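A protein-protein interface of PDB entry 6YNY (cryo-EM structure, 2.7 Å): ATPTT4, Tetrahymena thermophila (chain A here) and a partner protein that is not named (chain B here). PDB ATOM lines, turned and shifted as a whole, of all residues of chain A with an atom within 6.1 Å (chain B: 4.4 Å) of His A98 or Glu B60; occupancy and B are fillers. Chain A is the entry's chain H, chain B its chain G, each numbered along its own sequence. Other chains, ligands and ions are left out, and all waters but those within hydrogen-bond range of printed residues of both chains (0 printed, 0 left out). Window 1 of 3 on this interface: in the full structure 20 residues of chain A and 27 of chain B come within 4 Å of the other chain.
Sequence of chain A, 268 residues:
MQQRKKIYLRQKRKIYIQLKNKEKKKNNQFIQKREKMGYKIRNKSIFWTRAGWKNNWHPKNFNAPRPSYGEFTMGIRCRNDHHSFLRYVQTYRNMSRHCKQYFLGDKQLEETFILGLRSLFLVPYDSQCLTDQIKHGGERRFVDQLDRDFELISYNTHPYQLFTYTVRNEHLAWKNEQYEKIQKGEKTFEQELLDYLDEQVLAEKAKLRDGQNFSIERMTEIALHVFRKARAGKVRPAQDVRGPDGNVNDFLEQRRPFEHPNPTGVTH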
ATOM      1  N   GLN A  90      -5.698 -12.498  -1.098  1.00  0.00           N
ATOM      2  CA  GLN A  90      -5.480 -12.076   0.279  1.00  0.00           C
ATOM      3  C   GLN A  90      -6.646 -12.464   1.175  1.00  0.00           C
ATOM      4  O   GLN A  90      -6.452 -12.723   2.367  1.00  0.00           O
ATOM      5  CB  GLN A  90      -5.252 -10.569   0.324  1.00  0.00           C
ATOM      6  CG  GLN A  90      -4.849 -10.044   1.674  1.00  0.00           C
ATOM      7  CD  GLN A  90      -3.557 -10.640   2.166  1.00  0.00           C
ATOM      8  OE1 GLN A  90      -2.739 -11.115   1.381  1.00  0.00           O
ATOM      9  NE2 GLN A  90      -3.368 -10.631   3.473  1.00  0.00           N
ATOM     10  N   ARG A  93      -6.094 -16.033   2.340  1.00  0.00           N
ATOM     11  CA  ARG A  93      -5.028 -16.148   3.327  1.00  0.00           C
ATOM     12  C   ARG A  93      -5.491 -15.674   4.698  1.00  0.00           C
ATOM     13  O   ARG A  93      -5.092 -16.238   5.723  1.00  0.00           O
ATOM     14  CB  ARG A  93      -3.814 -15.351   2.866  1.00  0.00           C
ATOM     15  CG  ARG A  93      -2.571 -15.593   3.679  1.00  0.00           C
ATOM     16  CD  ARG A  93      -2.039 -14.310   4.247  1.00  0.00           C
ATOM     17  NE  ARG A  93      -1.698 -13.350   3.203  1.00  0.00           N
ATOM     18  CZ  ARG A  93      -0.503 -13.251   2.630  1.00  0.00           C
ATOM     19  NH1 ARG A  93       0.489 -14.049   2.985  1.00  0.00           N
ATOM     20  NH2 ARG A  93      -0.302 -12.345   1.693  1.00  0.00           N
ATOM     21  N   ASN A  94      -6.328 -14.641   4.738  1.00  0.00           N
ATOM     22  CA  ASN A  94      -6.798 -14.119   6.014  1.00  0.00           C
ATOM     23  C   ASN A  94      -7.814 -15.057   6.648  1.00  0.00           C
ATOM     24  O   ASN A  94      -7.730 -15.366   7.842  1.00  0.00           O
ATOM     25  CB  ASN A  94      -7.405 -12.733   5.823  1.00  0.00           C
ATOM     26  CG  ASN A  94      -6.406 -11.718   5.345  1.00  0.00           C
ATOM     27  OD1 ASN A  94      -5.198 -11.917   5.438  1.00  0.00           O
ATOM     28  ND2 ASN A  94      -6.911 -10.608   4.841  1.00  0.00           N
ATOM     29  N   MET A  95      -8.795 -15.511   5.867  1.00  0.00           N
ATOM     30  CA  MET A  95      -9.811 -16.405   6.405  1.00  0.00           C
ATOM     31  C   MET A  95      -9.193 -17.690   6.932  1.00  0.00           C
ATOM     32  O   MET A  95      -9.665 -18.242   7.931  1.00  0.00           O
ATOM     33  CB  MET A  95     -10.846 -16.709   5.327  1.00  0.00           C
ATOM     34  CG  MET A  95     -11.586 -15.480   4.857  1.00  0.00           C
ATOM     35  SD  MET A  95     -12.600 -15.725   3.395  1.00  0.00           S
ATOM     36  CE  MET A  95     -13.907 -16.725   4.071  1.00  0.00           C
ATOM     37  N   SER A  96      -8.138 -18.173   6.282  1.00  0.00           N
ATOM     38  CA  SER A  96      -7.469 -19.380   6.748  1.00  0.00           C
ATOM     39  C   SER A  96      -6.652 -19.101   7.998  1.00  0.00           C
ATOM     40  O   SER A  96      -6.743 -19.831   8.991  1.00  0.00           O
ATOM     41  CB  SER A  96      -6.575 -19.934   5.643  1.00  0.00           C
ATOM     42  OG  SER A  96      -5.887 -21.089   6.076  1.00  0.00           O
ATOM     43  N   ARG A  97      -5.851 -18.039   7.967  1.00  0.00           N
ATOM     44  CA  ARG A  97      -4.943 -17.757   9.069  1.00  0.00           C
ATOM     45  C   ARG A  97      -5.681 -17.248  10.299  1.00  0.00           C
ATOM     46  O   ARG A  97      -5.235 -17.485  11.427  1.00  0.00           O
ATOM     47  CB  ARG A  97      -3.895 -16.751   8.608  1.00  0.00           C
ATOM     48  CG  ARG A  97      -2.906 -16.348   9.653  1.00  0.00           C
ATOM     49  CD  ARG A  97      -1.833 -15.486   9.050  1.00  0.00           C
ATOM     50  NE  ARG A  97      -0.907 -16.241   8.216  1.00  0.00           N
ATOM     51  CZ  ARG A  97      -0.048 -15.687   7.371  1.00  0.00           C
ATOM     52  NH1 ARG A  97       0.759 -16.450   6.656  1.00  0.00           N
ATOM     53  NH2 ARG A  97       0.001 -14.372   7.230  1.00  0.00           N
ATOM     54  N   HIS A  98      -6.805 -16.558  10.111  1.00  0.00           N
ATOM     55  CA  HIS A  98      -7.549 -16.035  11.250  1.00  0.00           C
ATOM     56  C   HIS A  98      -8.442 -17.086  11.893  1.00  0.00           C
ATOM     57  O   HIS A  98      -8.765 -16.973  13.079  1.00  0.00           O
ATOM     58  CB  HIS A  98      -8.386 -14.829  10.826  1.00  0.00           C
ATOM     59  CG  HIS A  98      -7.594 -13.574  10.645  1.00  0.00           C
ATOM     60  ND1 HIS A  98      -7.718 -12.493  11.487  1.00  0.00           N
ATOM     61  CD2 HIS A  98      -6.663 -13.227   9.724  1.00  0.00           C
ATOM     62  CE1 HIS A  98      -6.903 -11.533  11.092  1.00  0.00           C
ATOM     63  NE2 HIS A  98      -6.250 -11.954  10.024  1.00  0.00           N
ATOM     64  N   CYS A  99      -8.857 -18.105  11.140  1.00  0.00           N
ATOM     65  CA  CYS A  99      -9.633 -19.187  11.730  1.00  0.00           C
ATOM     66  C   CYS A  99      -8.747 -20.205  12.434  1.00  0.00           C
ATOM     67  O   CYS A  99      -9.191 -20.842  13.395  1.00  0.00           O
ATOM     68  CB  CYS A  99     -10.472 -19.880  10.659  1.00  0.00           C
ATOM     69  SG  CYS A  99     -11.910 -18.950  10.117  1.00  0.00           S
ATOM     70  N   LYS A 100      -7.504 -20.368  11.981  1.00  0.00           N
ATOM     71  CA  LYS A 100      -6.578 -21.290  12.623  1.00  0.00           C
ATOM     72  C   LYS A 100      -6.150 -20.829  14.004  1.00  0.00           C
ATOM     73  O   LYS A 100      -5.567 -21.621  14.749  1.00  0.00           O
ATOM     74  CB  LYS A 100      -5.344 -21.483  11.752  1.00  0.00           C
ATOM     75  CG  LYS A 100      -5.582 -22.333  10.529  1.00  0.00           C
ATOM     76  CD  LYS A 100      -4.346 -22.402   9.669  1.00  0.00           C
ATOM     77  CE  LYS A 100      -4.614 -23.126   8.370  1.00  0.00           C
ATOM     78  NZ  LYS A 100      -3.433 -23.088   7.476  1.00  0.00           N
ATOM     79  N   GLN A 101      -6.420 -19.574  14.360  1.00  0.00           N
ATOM     80  CA  GLN A 101      -6.067 -19.091  15.686  1.00  0.00           C
ATOM     81  C   GLN A 101      -6.778 -19.875  16.776  1.00  0.00           C
ATOM     82  O   GLN A 101      -6.266 -19.984  17.895  1.00  0.00           O
ATOM     83  CB  GLN A 101      -6.405 -17.608  15.796  1.00  0.00           C
ATOM     84  CG  GLN A 101      -6.197 -17.028  17.173  1.00  0.00           C
ATOM     85  CD  GLN A 101      -6.311 -15.519  17.207  1.00  0.00           C
ATOM     86  OE1 GLN A 101      -5.706 -14.861  18.051  1.00  0.00           O
ATOM     87  NE2 GLN A 101      -7.088 -14.962  16.295  1.00  0.00           N
ATOM     88  N   TYR A 102      -7.945 -20.435  16.469  1.00  0.00           N
ATOM     89  CA  TYR A 102      -8.791 -21.078  17.460  1.00  0.00           C
ATOM     90  C   TYR A 102      -8.877 -22.587  17.268  1.00  0.00           C
ATOM     91  O   TYR A 102      -9.771 -23.228  17.828  1.00  0.00           O
ATOM     92  CB  TYR A 102     -10.184 -20.460  17.423  1.00  0.00           C
ATOM     93  CG  TYR A 102     -10.195 -18.975  17.676  1.00  0.00           C
ATOM     94  CD1 TYR A 102     -10.093 -18.471  18.959  1.00  0.00           C
ATOM     95  CD2 TYR A 102     -10.311 -18.075  16.631  1.00  0.00           C
ATOM     96  CE1 TYR A 102     -10.102 -17.124  19.193  1.00  0.00           C
ATOM     97  CE2 TYR A 102     -10.322 -16.723  16.860  1.00  0.00           C
ATOM     98  CZ  TYR A 102     -10.217 -16.253  18.142  1.00  0.00           C
ATOM     99  OH  TYR A 102     -10.227 -14.902  18.379  1.00  0.00           O
ATOM    100  N   PHE A 150     -15.202 -12.646   6.047  1.00  0.00           N
ATOM    101  CA  PHE A 150     -13.978 -12.502   6.826  1.00  0.00           C
ATOM    102  C   PHE A 150     -14.163 -11.519   7.974  1.00  0.00           C
ATOM    103  O   PHE A 150     -13.594 -11.708   9.055  1.00  0.00           O
ATOM    104  CB  PHE A 150     -12.830 -12.055   5.929  1.00  0.00           C
ATOM    105  CG  PHE A 150     -11.626 -11.604   6.687  1.00  0.00           C
ATOM    106  CD1 PHE A 150     -10.983 -12.461   7.554  1.00  0.00           C
ATOM    107  CD2 PHE A 150     -11.140 -10.324   6.542  1.00  0.00           C
ATOM    108  CE1 PHE A 150      -9.885 -12.049   8.257  1.00  0.00           C
ATOM    109  CE2 PHE A 150     -10.036  -9.912   7.244  1.00  0.00           C
ATOM    110  CZ  PHE A 150      -9.409 -10.775   8.101  1.00  0.00           C
ATOM    111  N   ILE A 153     -15.249 -13.454  10.630  1.00  0.00           N
ATOM    112  CA  ILE A 153     -14.204 -14.378  11.049  1.00  0.00           C
ATOM    113  C   ILE A 153     -13.166 -13.665  11.903  1.00  0.00           C
ATOM    114  O   ILE A 153     -12.605 -14.247  12.838  1.00  0.00           O
ATOM    115  CB  ILE A 153     -13.572 -15.038   9.813  1.00  0.00           C
ATOM    116  CG1 ILE A 153     -14.559 -16.023   9.193  1.00  0.00           C
ATOM    117  CG2 ILE A 153     -12.270 -15.714  10.168  1.00  0.00           C
ATOM    118  CD1 ILE A 153     -14.157 -16.520   7.848  1.00  0.00           C
ATOM    119  N   SER A 154     -12.888 -12.399  11.594  1.00  0.00           N
ATOM    120  CA  SER A 154     -11.920 -11.646  12.379  1.00  0.00           C
ATOM    121  C   SER A 154     -12.382 -11.470  13.817  1.00  0.00           C
ATOM    122  O   SER A 154     -11.552 -11.368  14.726  1.00  0.00           O
ATOM    123  CB  SER A 154     -11.669 -10.289  11.730  1.00  0.00           C
ATOM    124  OG  SER A 154     -12.865  -9.546  11.630  1.00  0.00           O
ATOM    125  N   GLN A 161     -17.530 -21.001  12.111  1.00  0.00           N
ATOM    126  CA  GLN A 161     -16.582 -21.176  13.202  1.00  0.00           C
ATOM    127  C   GLN A 161     -17.237 -21.858  14.394  1.00  0.00           C
ATOM    128  O   GLN A 161     -16.741 -22.872  14.896  1.00  0.00           O
ATOM    129  CB  GLN A 161     -16.016 -19.822  13.617  1.00  0.00           C
ATOM    130  CG  GLN A 161     -15.266 -19.093  12.533  1.00  0.00           C
ATOM    131  CD  GLN A 161     -14.872 -17.697  12.948  1.00  0.00           C
ATOM    132  OE1 GLN A 161     -15.721 -16.834  13.153  1.00  0.00           O
ATOM    133  NE2 GLN A 161     -13.579 -17.469  13.079  1.00  0.00           N
ATOM    134  N   ASN B  38      -1.578  -2.037   9.084  1.00  0.00           N
ATOM    135  CA  ASN B  38      -1.730  -3.307   8.395  1.00  0.00           C
ATOM    136  C   ASN B  38      -0.441  -3.633   7.645  1.00  0.00           C
ATOM    137  O   ASN B  38       0.080  -2.777   6.922  1.00  0.00           O
ATOM    138  CB  ASN B  38      -2.911  -3.240   7.436  1.00  0.00           C
ATOM    139  CG  ASN B  38      -3.573  -4.580   7.234  1.00  0.00           C
ATOM    140  OD1 ASN B  38      -4.410  -4.996   8.034  1.00  0.00           O
ATOM    141  ND2 ASN B  38      -3.212  -5.260   6.159  1.00  0.00           N
ATOM    142  N   PRO B  39       0.102  -4.847   7.784  1.00  0.00           N
ATOM    143  CA  PRO B  39       1.430  -5.119   7.220  1.00  0.00           C
ATOM    144  C   PRO B  39       1.434  -5.507   5.753  1.00  0.00           C
ATOM    145  O   PRO B  39       2.476  -5.366   5.102  1.00  0.00           O
ATOM    146  CB  PRO B  39       1.932  -6.276   8.085  1.00  0.00           C
ATOM    147  CG  PRO B  39       0.696  -7.014   8.426  1.00  0.00           C
ATOM    148  CD  PRO B  39      -0.390  -5.984   8.578  1.00  0.00           C
ATOM    149  N   TYR B  40       0.323  -5.994   5.217  1.00  0.00           N
ATOM    150  CA  TYR B  40       0.273  -6.527   3.865  1.00  0.00           C
ATOM    151  C   TYR B  40      -0.237  -5.492   2.872  1.00  0.00           C
ATOM    152  O   TYR B  40      -1.031  -4.612   3.211  1.00  0.00           O
ATOM    153  CB  TYR B  40      -0.623  -7.763   3.801  1.00  0.00           C
ATOM    154  CG  TYR B  40      -0.044  -9.003   4.428  1.00  0.00           C
ATOM    155  CD1 TYR B  40       1.111  -9.575   3.933  1.00  0.00           C
ATOM    156  CD2 TYR B  40      -0.669  -9.616   5.498  1.00  0.00           C
ATOM    157  CE1 TYR B  40       1.639 -10.710   4.496  1.00  0.00           C
ATOM    158  CE2 TYR B  40      -0.152 -10.753   6.065  1.00  0.00           C
ATOM    159  CZ  TYR B  40       1.003 -11.298   5.561  1.00  0.00           C
ATOM    160  OH  TYR B  40       1.531 -12.435   6.119  1.00  0.00           O
ATOM    161  N   ASP B  58      -8.730  -7.397  14.303  1.00  0.00           N
ATOM    162  CA  ASP B  58      -7.284  -7.284  14.341  1.00  0.00           C
ATOM    163  C   ASP B  58      -6.752  -7.086  12.932  1.00  0.00           C
ATOM    164  O   ASP B  58      -7.369  -7.512  11.952  1.00  0.00           O
ATOM    165  CB  ASP B  58      -6.650  -8.534  14.957  1.00  0.00           C
ATOM    166  CG  ASP B  58      -7.300  -8.937  16.263  1.00  0.00           C
ATOM    167  OD1 ASP B  58      -7.761  -8.044  17.003  1.00  0.00           O
ATOM    168  OD2 ASP B  58      -7.356 -10.151  16.548  1.00  0.00           O
ATOM    169  N   TYR B  59      -5.602  -6.426  12.837  1.00  0.00           N
ATOM    170  CA  TYR B  59      -4.950  -6.283  11.551  1.00  0.00           C
ATOM    171  C   TYR B  59      -4.571  -7.656  11.007  1.00  0.00           C
ATOM    172  O   TYR B  59      -4.463  -8.639  11.743  1.00  0.00           O
ATOM    173  CB  TYR B  59      -3.713  -5.399  11.671  1.00  0.00           C
ATOM    174  CG  TYR B  59      -4.009  -4.008  12.168  1.00  0.00           C
ATOM    175  CD1 TYR B  59      -4.679  -3.095  11.372  1.00  0.00           C
ATOM    176  CD2 TYR B  59      -3.614  -3.607  13.430  1.00  0.00           C
ATOM    177  CE1 TYR B  59      -4.953  -1.827  11.825  1.00  0.00           C
ATOM    178  CE2 TYR B  59      -3.882  -2.342  13.891  1.00  0.00           C
ATOM    179  CZ  TYR B  59      -4.551  -1.454  13.085  1.00  0.00           C
ATOM    180  OH  TYR B  59      -4.818  -0.186  13.544  1.00  0.00           O
ATOM    181  N   GLU B  60      -4.374  -7.716   9.695  1.00  0.00           N
ATOM    182  CA  GLU B  60      -4.097  -8.984   9.037  1.00  0.00           C
ATOM    183  C   GLU B  60      -2.908  -9.674   9.688  1.00  0.00           C
ATOM    184  O   GLU B  60      -1.837  -9.085   9.841  1.00  0.00           O
ATOM    185  CB  GLU B  60      -3.839  -8.757   7.548  1.00  0.00           C
ATOM    186  CG  GLU B  60      -5.033  -8.190   6.807  1.00  0.00           C
ATOM    187  CD  GLU B  60      -4.805  -8.082   5.314  1.00  0.00           C
ATOM    188  OE1 GLU B  60      -5.675  -7.520   4.618  1.00  0.00           O
ATOM    189  OE2 GLU B  60      -3.758  -8.562   4.835  1.00  0.00           O
ATOM    190  N   HIS B  61      -3.111 -10.927  10.082  1.00  0.00           N
ATOM    191  CA  HIS B  61      -2.093 -11.669  10.803  1.00  0.00           C
ATOM    192  C   HIS B  61      -0.983 -12.116   9.865  1.00  0.00           C
ATOM    193  O   HIS B  61      -1.237 -12.592   8.756  1.00  0.00           O
ATOM    194  CB  HIS B  61      -2.709 -12.884  11.492  1.00  0.00           C
ATOM    195  CG  HIS B  61      -3.672 -12.540  12.581  1.00  0.00           C
ATOM    196  ND1 HIS B  61      -3.796 -11.266  13.089  1.00  0.00           N
ATOM    197  CD2 HIS B  61      -4.556 -13.304  13.264  1.00  0.00           C
ATOM    198  CE1 HIS B  61      -4.716 -11.261  14.037  1.00  0.00           C
ATOM    199  NE2 HIS B  61      -5.192 -12.486  14.162  1.00  0.00           N
ATOM    200  N   THR B  62       0.255 -11.966  10.324  1.00  0.00           N
ATOM    201  CA  THR B  62       1.419 -12.440   9.595  1.00  0.00           C
ATOM    202  C   THR B  62       1.778 -13.876   9.936  1.00  0.00           C
ATOM    203  O   THR B  62       2.627 -14.467   9.261  1.00  0.00           O
ATOM    204  CB  THR B  62       2.616 -11.534   9.878  1.00  0.00           C
ATOM    205  OG1 THR B  62       2.807 -11.420  11.293  1.00  0.00           O
ATOM    206  CG2 THR B  62       2.376 -10.165   9.299  1.00  0.00           C
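NH2 of Arg A97 is in hydrogen-bond range of OH of Tyr B40 (2.7 Å).
NE2 of Gln A90 sits at hydrogen-bond distance from OE2 of Glu B60, at 2.5 Å.
The side-chain amide nitrogen (ND2) of Asn A94 sits close to the side-chain carboxylate (OE1) of Glu B60, 3.3 Å away.
The guanidinium group (NH2) of Arg A97 sits at hydrogen-bond distance from the backbone carbonyl oxygen (O) of His B61 (2.7 Å).
The backbone NH (N) of His B61 sits at hydrogen-bond distance from a ring nitrogen (NE2) of His A98, at 3.3 Å.
O of Thr B62 sits close to NH2 of Arg A97.
The side-chain amide oxygen (OD1) of Asn B38 is in hydrogen-bond range of the backbone NH (N) of Glu B60, at 3.2 Å.
The backbone carbonyl oxygen of Tyr B59 sits at hydrogen-bond distance from a ring nitrogen (ND1) of His B61, at 3.0 Å.
The side-chain amide oxygen (OE1) of Gln A90 is in hydrogen-bond range of the guanidinium group (NH2) of Arg A93 (2.7 Å).
NE2 of Gln A90 lies within hydrogen-bond range of OD1 of Asn A94, 3.0 Å away.
Among the printed residues, pairs that only touch across the chains: Gln A90 with Tyr B40, Arg A93 with Tyr B40, Gln A101 with His B61, His A98 with Glu B60 and His A98 with Tyr B59.
His A98 touches just these residues of chain B: Tyr B59 (3.8 Å), Glu B60 (3.8 Å) and His B61 (3.3 Å).
Glu B60 touches three residues of chain A.
Printed residues of chain A within 4 Å of Tyr B59: His A98 (3.8 Å).
Of the printed residues of chain B, Arg A97 touches Tyr B40, His B61 and Thr B62.
Of the printed residues of chain A, Tyr B40 touches Gln A90 (3.5 Å), Arg A93 (3.7 Å) and Arg A97 (2.7 Å).
Printed residues of chain B within 4 Å of Arg A93: Tyr B40.
Of the printed residues of chain B, Gln A90 touches Tyr B40 (3.5 Å) and Glu B60 (2.5 Å).
Asn B38 touches none of the printed residues of chain A.
Ser A96 touches none of the printed residues of chain B.
Printed residues of chain A that touch a printed residue of chain B: Gln A90, Arg A93, Asn A94, Arg A97, His A98 and Gln A101.
Hydrophobic or aromatic side chains of chain A that line the printed part of chain B: His A98.
Of the 8 printed residues of chain B, 5 touch a printed residue of chain A.
Printed residues of chain B that touch a printed residue of chain A: Tyr B40, Tyr B59, Glu B60, His B61 and Thr B62.
Hydrophobic or aromatic side chains of chain B within 4 Å of the printed part of chain A: Tyr B40 and His B61.
Among the printed residues, no Asp or Glu carboxylate lies within 4 Å of a Lys or Arg side-chain nitrogen of the other chain.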
